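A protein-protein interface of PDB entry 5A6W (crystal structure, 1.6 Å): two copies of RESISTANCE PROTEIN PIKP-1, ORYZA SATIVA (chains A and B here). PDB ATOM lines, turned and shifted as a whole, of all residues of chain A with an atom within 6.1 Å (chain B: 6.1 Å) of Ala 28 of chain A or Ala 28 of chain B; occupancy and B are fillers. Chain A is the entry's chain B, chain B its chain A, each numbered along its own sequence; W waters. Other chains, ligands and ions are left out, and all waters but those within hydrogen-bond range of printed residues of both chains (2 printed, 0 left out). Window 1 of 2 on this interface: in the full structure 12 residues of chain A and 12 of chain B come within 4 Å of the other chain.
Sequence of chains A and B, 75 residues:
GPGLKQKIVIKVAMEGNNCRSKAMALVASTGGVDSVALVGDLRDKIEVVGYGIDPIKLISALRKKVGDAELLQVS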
ATOM      1  N   ARG A  20       8.596  21.760 -10.109  1.00  0.00           N
ATOM      2  CA  ARG A  20       9.840  21.026  -9.947  1.00  0.00           C
ATOM      3  C   ARG A  20      10.268  20.382 -11.257  1.00  0.00           C
ATOM      4  O   ARG A  20      11.402  20.590 -11.707  1.00  0.00           O
ATOM      5  CB  ARG A  20       9.686  19.954  -8.866  1.00  0.00           C
ATOM      6  CG  ARG A  20      10.960  19.177  -8.555  1.00  0.00           C
ATOM      7  CD  ARG A  20      10.802  18.357  -7.278  1.00  0.00           C
ATOM      8  NE  ARG A  20      10.672  19.232  -6.109  1.00  0.00           N
ATOM      9  CZ  ARG A  20      11.607  19.442  -5.182  1.00  0.00           C
ATOM     10  NH1 ARG A  20      12.781  18.819  -5.217  1.00  0.00           N
ATOM     11  NH2 ARG A  20      11.347  20.276  -4.184  1.00  0.00           N
ATOM     12  N   SER A  21       9.361  19.620 -11.871  1.00  0.00           N
ATOM     13  CA  SER A  21       9.665  18.990 -13.157  1.00  0.00           C
ATOM     14  C   SER A  21       9.859  20.056 -14.243  1.00  0.00           C
ATOM     15  O   SER A  21      10.722  19.903 -15.103  1.00  0.00           O
ATOM     16  CB  SER A  21       8.613  17.934 -13.560  1.00  0.00           C
ATOM     17  OG  SER A  21       7.487  18.496 -14.211  1.00  0.00           O
ATOM     18  N   ALA A  23      11.034  23.152 -13.931  1.00  0.00           N
ATOM     19  CA  ALA A  23      12.340  23.781 -13.817  1.00  0.00           C
ATOM     20  C   ALA A  23      13.443  22.858 -14.317  1.00  0.00           C
ATOM     21  O   ALA A  23      14.339  23.284 -15.051  1.00  0.00           O
ATOM     22  CB  ALA A  23      12.622  24.215 -12.381  1.00  0.00           C
ATOM     23  N   MET A  24      13.382  21.590 -13.906  1.00  0.00           N
ATOM     24  CA  MET A  24      14.392  20.632 -14.329  1.00  0.00           C
ATOM     25  C   MET A  24      14.379  20.481 -15.825  1.00  0.00           C
ATOM     26  O   MET A  24      15.430  20.444 -16.465  1.00  0.00           O
ATOM     27  CB  MET A  24      14.115  19.269 -13.692  1.00  0.00           C
ATOM     28  CG  MET A  24      14.379  19.239 -12.193  1.00  0.00           C
ATOM     29  SD  MET A  24      16.139  19.301 -11.840  1.00  0.00           S
ATOM     30  CE  MET A  24      16.685  17.631 -12.221  1.00  0.00           C
ATOM     31  N   ALA A  25      13.184  20.364 -16.397  1.00  0.00           N
ATOM     32  CA  ALA A  25      13.082  20.182 -17.847  1.00  0.00           C
ATOM     33  C   ALA A  25      13.632  21.392 -18.596  1.00  0.00           C
ATOM     34  O   ALA A  25      14.381  21.243 -19.563  1.00  0.00           O
ATOM     35  CB  ALA A  25      11.636  19.900 -18.242  1.00  0.00           C
ATOM     36  N   LEU A  26      13.298  22.596 -18.138  1.00  0.00           N
ATOM     37  CA  LEU A  26      13.821  23.822 -18.763  1.00  0.00           C
ATOM     38  C   LEU A  26      15.335  23.871 -18.739  1.00  0.00           C
ATOM     39  O   LEU A  26      15.975  24.117 -19.748  1.00  0.00           O
ATOM     40  CB  LEU A  26      13.240  25.082 -18.080  1.00  0.00           C
ATOM     41  CG  LEU A  26      13.584  26.435 -18.719  1.00  0.00           C
ATOM     42  CD1 LEU A  26      12.503  27.458 -18.386  1.00  0.00           C
ATOM     43  CD2 LEU A  26      14.962  26.960 -18.316  1.00  0.00           C
ATOM     44  N   VAL A  27      15.918  23.617 -17.580  1.00  0.00           N
ATOM     45  CA  VAL A  27      17.383  23.660 -17.443  1.00  0.00           C
ATOM     46  C   VAL A  27      17.987  22.570 -18.322  1.00  0.00           C
ATOM     47  O   VAL A  27      18.930  22.812 -19.048  1.00  0.00           O
ATOM     48  CB  VAL A  27      17.815  23.500 -15.971  1.00  0.00           C
ATOM     49  CG1 VAL A  27      19.314  23.388 -15.876  1.00  0.00           C
ATOM     50  CG2 VAL A  27      17.331  24.680 -15.150  1.00  0.00           C
ATOM     51  N   ALA A  28      17.430  21.355 -18.270  1.00  0.00           N
ATOM     52  CA  ALA A  28      17.997  20.256 -19.028  1.00  0.00           C
ATOM     53  C   ALA A  28      17.930  20.461 -20.517  1.00  0.00           C
ATOM     54  O   ALA A  28      18.745  19.903 -21.244  1.00  0.00           O
ATOM     55  CB  ALA A  28      17.328  18.931 -18.658  1.00  0.00           C
ATOM     56  N   SER A  29      16.922  21.207 -20.980  1.00  0.00           N
ATOM     57  CA  SER A  29      16.772  21.530 -22.406  1.00  0.00           C
ATOM     58  C   SER A  29      17.741  22.602 -22.928  1.00  0.00           C
ATOM     59  O   SER A  29      17.812  22.813 -24.132  1.00  0.00           O
ATOM     60  CB  SER A  29      15.328  22.000 -22.683  1.00  0.00           C
ATOM     61  OG  SER A  29      15.211  23.363 -22.304  1.00  0.00           O
ATOM     62  N   THR A  30      18.459  23.276 -22.027  1.00  0.00           N
ATOM     63  CA  THR A  30      19.325  24.399 -22.371  1.00  0.00           C
ATOM     64  C   THR A  30      20.608  23.947 -23.086  1.00  0.00           C
ATOM     65  O   THR A  30      21.249  22.933 -22.756  1.00  0.00           O
ATOM     66  CB  THR A  30      19.606  25.231 -21.109  1.00  0.00           C
ATOM     67  OG1 THR A  30      18.347  25.666 -20.586  1.00  0.00           O
ATOM     68  CG2 THR A  30      20.469  26.459 -21.427  1.00  0.00           C
ATOM     69  N   GLY A  31      20.962  24.683 -24.130  1.00  0.00           N
ATOM     70  CA  GLY A  31      22.131  24.343 -24.889  1.00  0.00           C
ATOM     71  C   GLY A  31      23.377  24.326 -24.023  1.00  0.00           C
ATOM     72  O   GLY A  31      23.581  25.206 -23.195  1.00  0.00           O
ATOM     73  N   VAL A  33      24.234  22.019 -21.814  1.00  0.00           N
ATOM     74  CA  VAL A  33      24.060  21.296 -20.533  1.00  0.00           C
ATOM     75  C   VAL A  33      24.526  19.848 -20.603  1.00  0.00           C
ATOM     76  O   VAL A  33      24.113  19.070 -21.486  1.00  0.00           O
ATOM     77  CB  VAL A  33      22.603  21.464 -19.992  1.00  0.00           C
ATOM     78  CG1 VAL A  33      22.317  20.552 -18.801  1.00  0.00           C
ATOM     79  CG2 VAL A  33      22.337  22.898 -19.633  1.00  0.00           C
ATOM     80  N   VAL A  36      22.195  17.882 -14.750  1.00  0.00           N
ATOM     81  CA  VAL A  36      21.372  18.711 -13.883  1.00  0.00           C
ATOM     82  C   VAL A  36      20.959  17.859 -12.703  1.00  0.00           C
ATOM     83  O   VAL A  36      20.601  16.679 -12.875  1.00  0.00           O
ATOM     84  CB  VAL A  36      20.092  19.127 -14.617  1.00  0.00           C
ATOM     85  CG1 VAL A  36      19.225  20.023 -13.755  1.00  0.00           C
ATOM     86  CG2 VAL A  36      20.451  19.784 -15.935  1.00  0.00           C
ATOM     87  N   ARG B  20      19.749  15.298 -28.276  1.00  0.00           N
ATOM     88  CA  ARG B  20      20.303  15.220 -26.923  1.00  0.00           C
ATOM     89  C   ARG B  20      19.520  16.100 -25.949  1.00  0.00           C
ATOM     90  O   ARG B  20      19.098  15.626 -24.883  1.00  0.00           O
ATOM     91  CB  ARG B  20      21.792  15.569 -26.917  1.00  0.00           C
ATOM     92  CG  ARG B  20      22.659  14.424 -27.419  1.00  0.00           C
ATOM     93  CD  ARG B  20      24.072  14.879 -27.729  1.00  0.00           C
ATOM     94  NE  ARG B  20      24.879  13.802 -28.300  1.00  0.00           N
ATOM     95  CZ  ARG B  20      24.811  13.376 -29.568  1.00  0.00           C
ATOM     96  NH1 ARG B  20      23.950  13.910 -30.439  1.00  0.00           N
ATOM     97  NH2 ARG B  20      25.607  12.393 -29.972  1.00  0.00           N
ATOM     98  N   SER B  21      19.312  17.366 -26.308  1.00  0.00           N
ATOM     99  CA  SER B  21      18.561  18.279 -25.443  1.00  0.00           C
ATOM    100  C   SER B  21      17.132  17.798 -25.265  1.00  0.00           C
ATOM    101  O   SER B  21      16.588  17.822 -24.156  1.00  0.00           O
ATOM    102  CB  SER B  21      18.566  19.704 -25.985  1.00  0.00           C
ATOM    103  OG  SER B  21      19.867  20.252 -25.918  1.00  0.00           O
ATOM    104  N   ALA B  23      16.026  14.674 -25.508  1.00  0.00           N
ATOM    105  CA  ALA B  23      16.091  13.499 -24.640  1.00  0.00           C
ATOM    106  C   ALA B  23      16.257  13.907 -23.182  1.00  0.00           C
ATOM    107  O   ALA B  23      15.608  13.371 -22.283  1.00  0.00           O
ATOM    108  CB  ALA B  23      17.256  12.598 -25.053  1.00  0.00           C
ATOM    109  N   MET B  24      17.163  14.850 -22.954  1.00  0.00           N
ATOM    110  CA  MET B  24      17.442  15.283 -21.588  1.00  0.00           C
ATOM    111  C   MET B  24      16.228  15.949 -20.944  1.00  0.00           C
ATOM    112  O   MET B  24      15.920  15.707 -19.788  1.00  0.00           O
ATOM    113  CB  MET B  24      18.640  16.252 -21.569  1.00  0.00           C
ATOM    114  CG  MET B  24      19.964  15.544 -21.811  1.00  0.00           C
ATOM    115  SD  MET B  24      20.555  14.688 -20.344  1.00  0.00           S
ATOM    116  CE  MET B  24      21.307  16.064 -19.481  1.00  0.00           C
ATOM    117  N   ALA B  25      15.559  16.820 -21.686  1.00  0.00           N
ATOM    118  CA  ALA B  25      14.386  17.500 -21.151  1.00  0.00           C
ATOM    119  C   ALA B  25      13.290  16.520 -20.826  1.00  0.00           C
ATOM    120  O   ALA B  25      12.643  16.629 -19.792  1.00  0.00           O
ATOM    121  CB  ALA B  25      13.875  18.554 -22.125  1.00  0.00           C
ATOM    122  N   LEU B  26      13.068  15.564 -21.722  1.00  0.00           N
ATOM    123  CA  LEU B  26      12.036  14.566 -21.497  1.00  0.00           C
ATOM    124  C   LEU B  26      12.307  13.799 -20.211  1.00  0.00           C
ATOM    125  O   LEU B  26      11.431  13.643 -19.370  1.00  0.00           O
ATOM    126  CB  LEU B  26      11.961  13.618 -22.692  1.00  0.00           C
ATOM    127  CG  LEU B  26      10.854  12.571 -22.679  1.00  0.00           C
ATOM    128  CD1 LEU B  26      10.613  12.087 -24.101  1.00  0.00           C
ATOM    129  CD2 LEU B  26      11.169  11.397 -21.765  1.00  0.00           C
ATOM    130  N   VAL B  27      13.521  13.300 -20.068  1.00  0.00           N
ATOM    131  CA  VAL B  27      13.845  12.504 -18.889  1.00  0.00           C
ATOM    132  C   VAL B  27      13.727  13.376 -17.637  1.00  0.00           C
ATOM    133  O   VAL B  27      13.138  12.967 -16.618  1.00  0.00           O
ATOM    134  CB  VAL B  27      15.229  11.862 -19.024  1.00  0.00           C
ATOM    135  CG1 VAL B  27      15.605  11.141 -17.745  1.00  0.00           C
ATOM    136  CG2 VAL B  27      15.237  10.867 -20.180  1.00  0.00           C
ATOM    137  N   ALA B  28      14.236  14.604 -17.723  1.00  0.00           N
ATOM    138  CA  ALA B  28      14.246  15.489 -16.566  1.00  0.00           C
ATOM    139  C   ALA B  28      12.830  15.837 -16.119  1.00  0.00           C
ATOM    140  O   ALA B  28      12.596  16.109 -14.943  1.00  0.00           O
ATOM    141  CB  ALA B  28      15.044  16.762 -16.867  1.00  0.00           C
ATOM    142  N   SER B  29      11.887  15.829 -17.060  1.00  0.00           N
ATOM    143  CA  SER B  29      10.494  16.154 -16.774  1.00  0.00           C
ATOM    144  C   SER B  29       9.734  14.997 -16.113  1.00  0.00           C
ATOM    145  O   SER B  29       8.607  15.167 -15.671  1.00  0.00           O
ATOM    146  CB  SER B  29       9.782  16.519 -18.084  1.00  0.00           C
ATOM    147  OG  SER B  29       9.527  15.347 -18.852  1.00  0.00           O
ATOM    148  N   THR B  30      10.352  13.828 -16.044  1.00  0.00           N
ATOM    149  CA  THR B  30       9.692  12.610 -15.570  1.00  0.00           C
ATOM    150  C   THR B  30       9.541  12.602 -14.048  1.00  0.00           C
ATOM    151  O   THR B  30      10.417  13.082 -13.320  1.00  0.00           O
ATOM    152  CB  THR B  30      10.483  11.376 -16.032  1.00  0.00           C
ATOM    153  OG1 THR B  30      10.611  11.408 -17.457  1.00  0.00           O
ATOM    154  CG2 THR B  30       9.814  10.066 -15.590  1.00  0.00           C
ATOM    155  N   GLY B  31       8.423  12.055 -13.561  1.00  0.00           N
ATOM    156  CA  GLY B  31       8.155  12.002 -12.124  1.00  0.00           C
ATOM    157  C   GLY B  31       9.208  11.191 -11.378  1.00  0.00           C
ATOM    158  O   GLY B  31       9.629  10.135 -11.842  1.00  0.00           O
ATOM    159  N   VAL B  33      12.356  11.937 -10.813  1.00  0.00           N
ATOM    160  CA  VAL B  33      13.755  12.187 -11.230  1.00  0.00           C
ATOM    161  C   VAL B  33      14.441  13.285 -10.378  1.00  0.00           C
ATOM    162  O   VAL B  33      13.951  14.420 -10.266  1.00  0.00           O
ATOM    163  CB  VAL B  33      13.854  12.478 -12.757  1.00  0.00           C
ATOM    164  CG1 VAL B  33      15.288  12.858 -13.182  1.00  0.00           C
ATOM    165  CG2 VAL B  33      13.377  11.250 -13.541  1.00  0.00           C
ATOM    166  N   VAL B  36      19.803  14.075 -13.959  1.00  0.00           N
ATOM    167  CA  VAL B  36      20.034  13.536 -15.298  1.00  0.00           C
ATOM    168  C   VAL B  36      21.386  13.965 -15.798  1.00  0.00           C
ATOM    169  O   VAL B  36      21.811  15.113 -15.572  1.00  0.00           O
ATOM    170  CB  VAL B  36      19.022  14.013 -16.363  1.00  0.00           C
ATOM    171  CG1 VAL B  36      17.718  13.268 -16.243  1.00  0.00           C
ATOM    172  CG2 VAL B  36      18.812  15.524 -16.341  1.00  0.00           C
HETATM  173  O   HOH W   1      20.346  20.481 -23.290  1.00  0.00           O
HETATM  174  O   HOH W   2      19.213  23.136 -26.718  1.00  0.00           O
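Printed residues of chain B that touch a printed residue of chain A: Ser 21, Met 24, Ala 25, Ala 28, Ser 29 and Val 36. Of the 13 printed residues of chain A, 6 touch a printed residue of chain B. Printed residues of chain A that touch a printed residue of chain B: Ser 21, Met 24, Ala 25, Ala 28, Ser 29 and Val 36. Hydrophobic or aromatic side chains of chain A within 4 Å of the printed part of chain B: Met 24, Ala 25 and Ala 28. Among the printed residues, no Asp or Glu carboxylate lies within 4 Å of a Lys or Arg side-chain nitrogen of the other chain.
The backbone carbonyl oxygen of Val 36 of chain B sits at hydrogen-bond distance from the backbone NH of Val 36 of chain A (2.9 Å).
Water W1 lies within hydrogen-bond range of O of Ala 28 of chain A (2.7 Å), O of Thr 30 of chain A (2.7 Å) and OG of Ser 21 of chain B (2.7 Å). Water W2 lies within hydrogen-bond range of O of Ser 29 of chain A, OG of Ser 21 of chain B and N of Gly 31 of chain A.
Met 24 of chain A touches Ala 28 of chain B, and with the chains exchanged Ala 28 of chain A touches Met 24 of chain B. Ala 25 of chain A touches its own counterpart, Ala 25 of chain B. Ala 25 of chain A touches Ser 29 of chain B, and with the chains exchanged Ser 29 of chain A touches Ala 25 of chain B. Ala 28 of chain B touches its own counterpart, Ala 28 of chain A.
O of Ser 29 of chain B touches CB of Ser 21 of chain A, at 3.5 Å. O of Ala 28 of chain B touches CB of Met 24 of chain A, at 3.7 Å. O of Ala 25 of chain A touches CB of Ala 25 of chain B (3.7 Å). CB of Ala 25 of chain A touches CB of Ser 29 of chain B, at 3.9 Å. Met 24 of chain B touches Ala 28 of chain A (CB to O, 3.7 Å). Ala 28 of chain B touches Ala 28 of chain A. Ser 21 of chain B touches Ser 29 of chain A. CB of Ser 29 of chain A touches CB of Ala 25 of chain B, at 3.8 Å.
O of Ala 25 of chain B lies close to OG of Ser 29 of chain B (3.5 Å). OG of Ser 29 of chain B is in hydrogen-bond range of O of Leu 26 of chain B, 2.6 Å away. The backbone carbonyl oxygen of Leu 26 of chain A is in hydrogen-bond range of the side-chain hydroxyl of Ser 29 of chain A, at 2.8 Å.
Arg 20 of chain A touches none of the printed residues of chain B. Printed residues of chain B within 4 Å of Met 24 of chain A: Ala 28 (3.7 Å). Printed residues of chain B within 4 Å of Ala 25 of chain A: Ala 25 and Ser 29. Ala 28 of chain A touches just these residues of chain B: Met 24 and Ala 28. Printed residues of chain B within 4 Å of Ser 29 of chain A: Ser 21 and Ala 25. Of the printed residues of chain A, Ala 25 of chain B touches Ala 25 and Ser 29. Leu 26 of chain B touches none of the printed residues of chain A. Of the printed residues of chain A, Ala 28 of chain B touches Met 24 and Ala 28. Of the printed residues of chain A, Ser 29 of chain B touches Ser 21 (3.5 Å) and Ala 25 (3.9 Å). The nearest residue of chain B that does not touch Ala 28 of chain A is Ala 25 of chain B (4.1 Å). The nearest residue of chain A that does not touch Ala 28 of chain B is Ala 25 of chain A (4.1 Å). The nearest printed residue of chain B that does not touch Ser 29 of chain A is Met 24 of chain B (5.3 Å).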
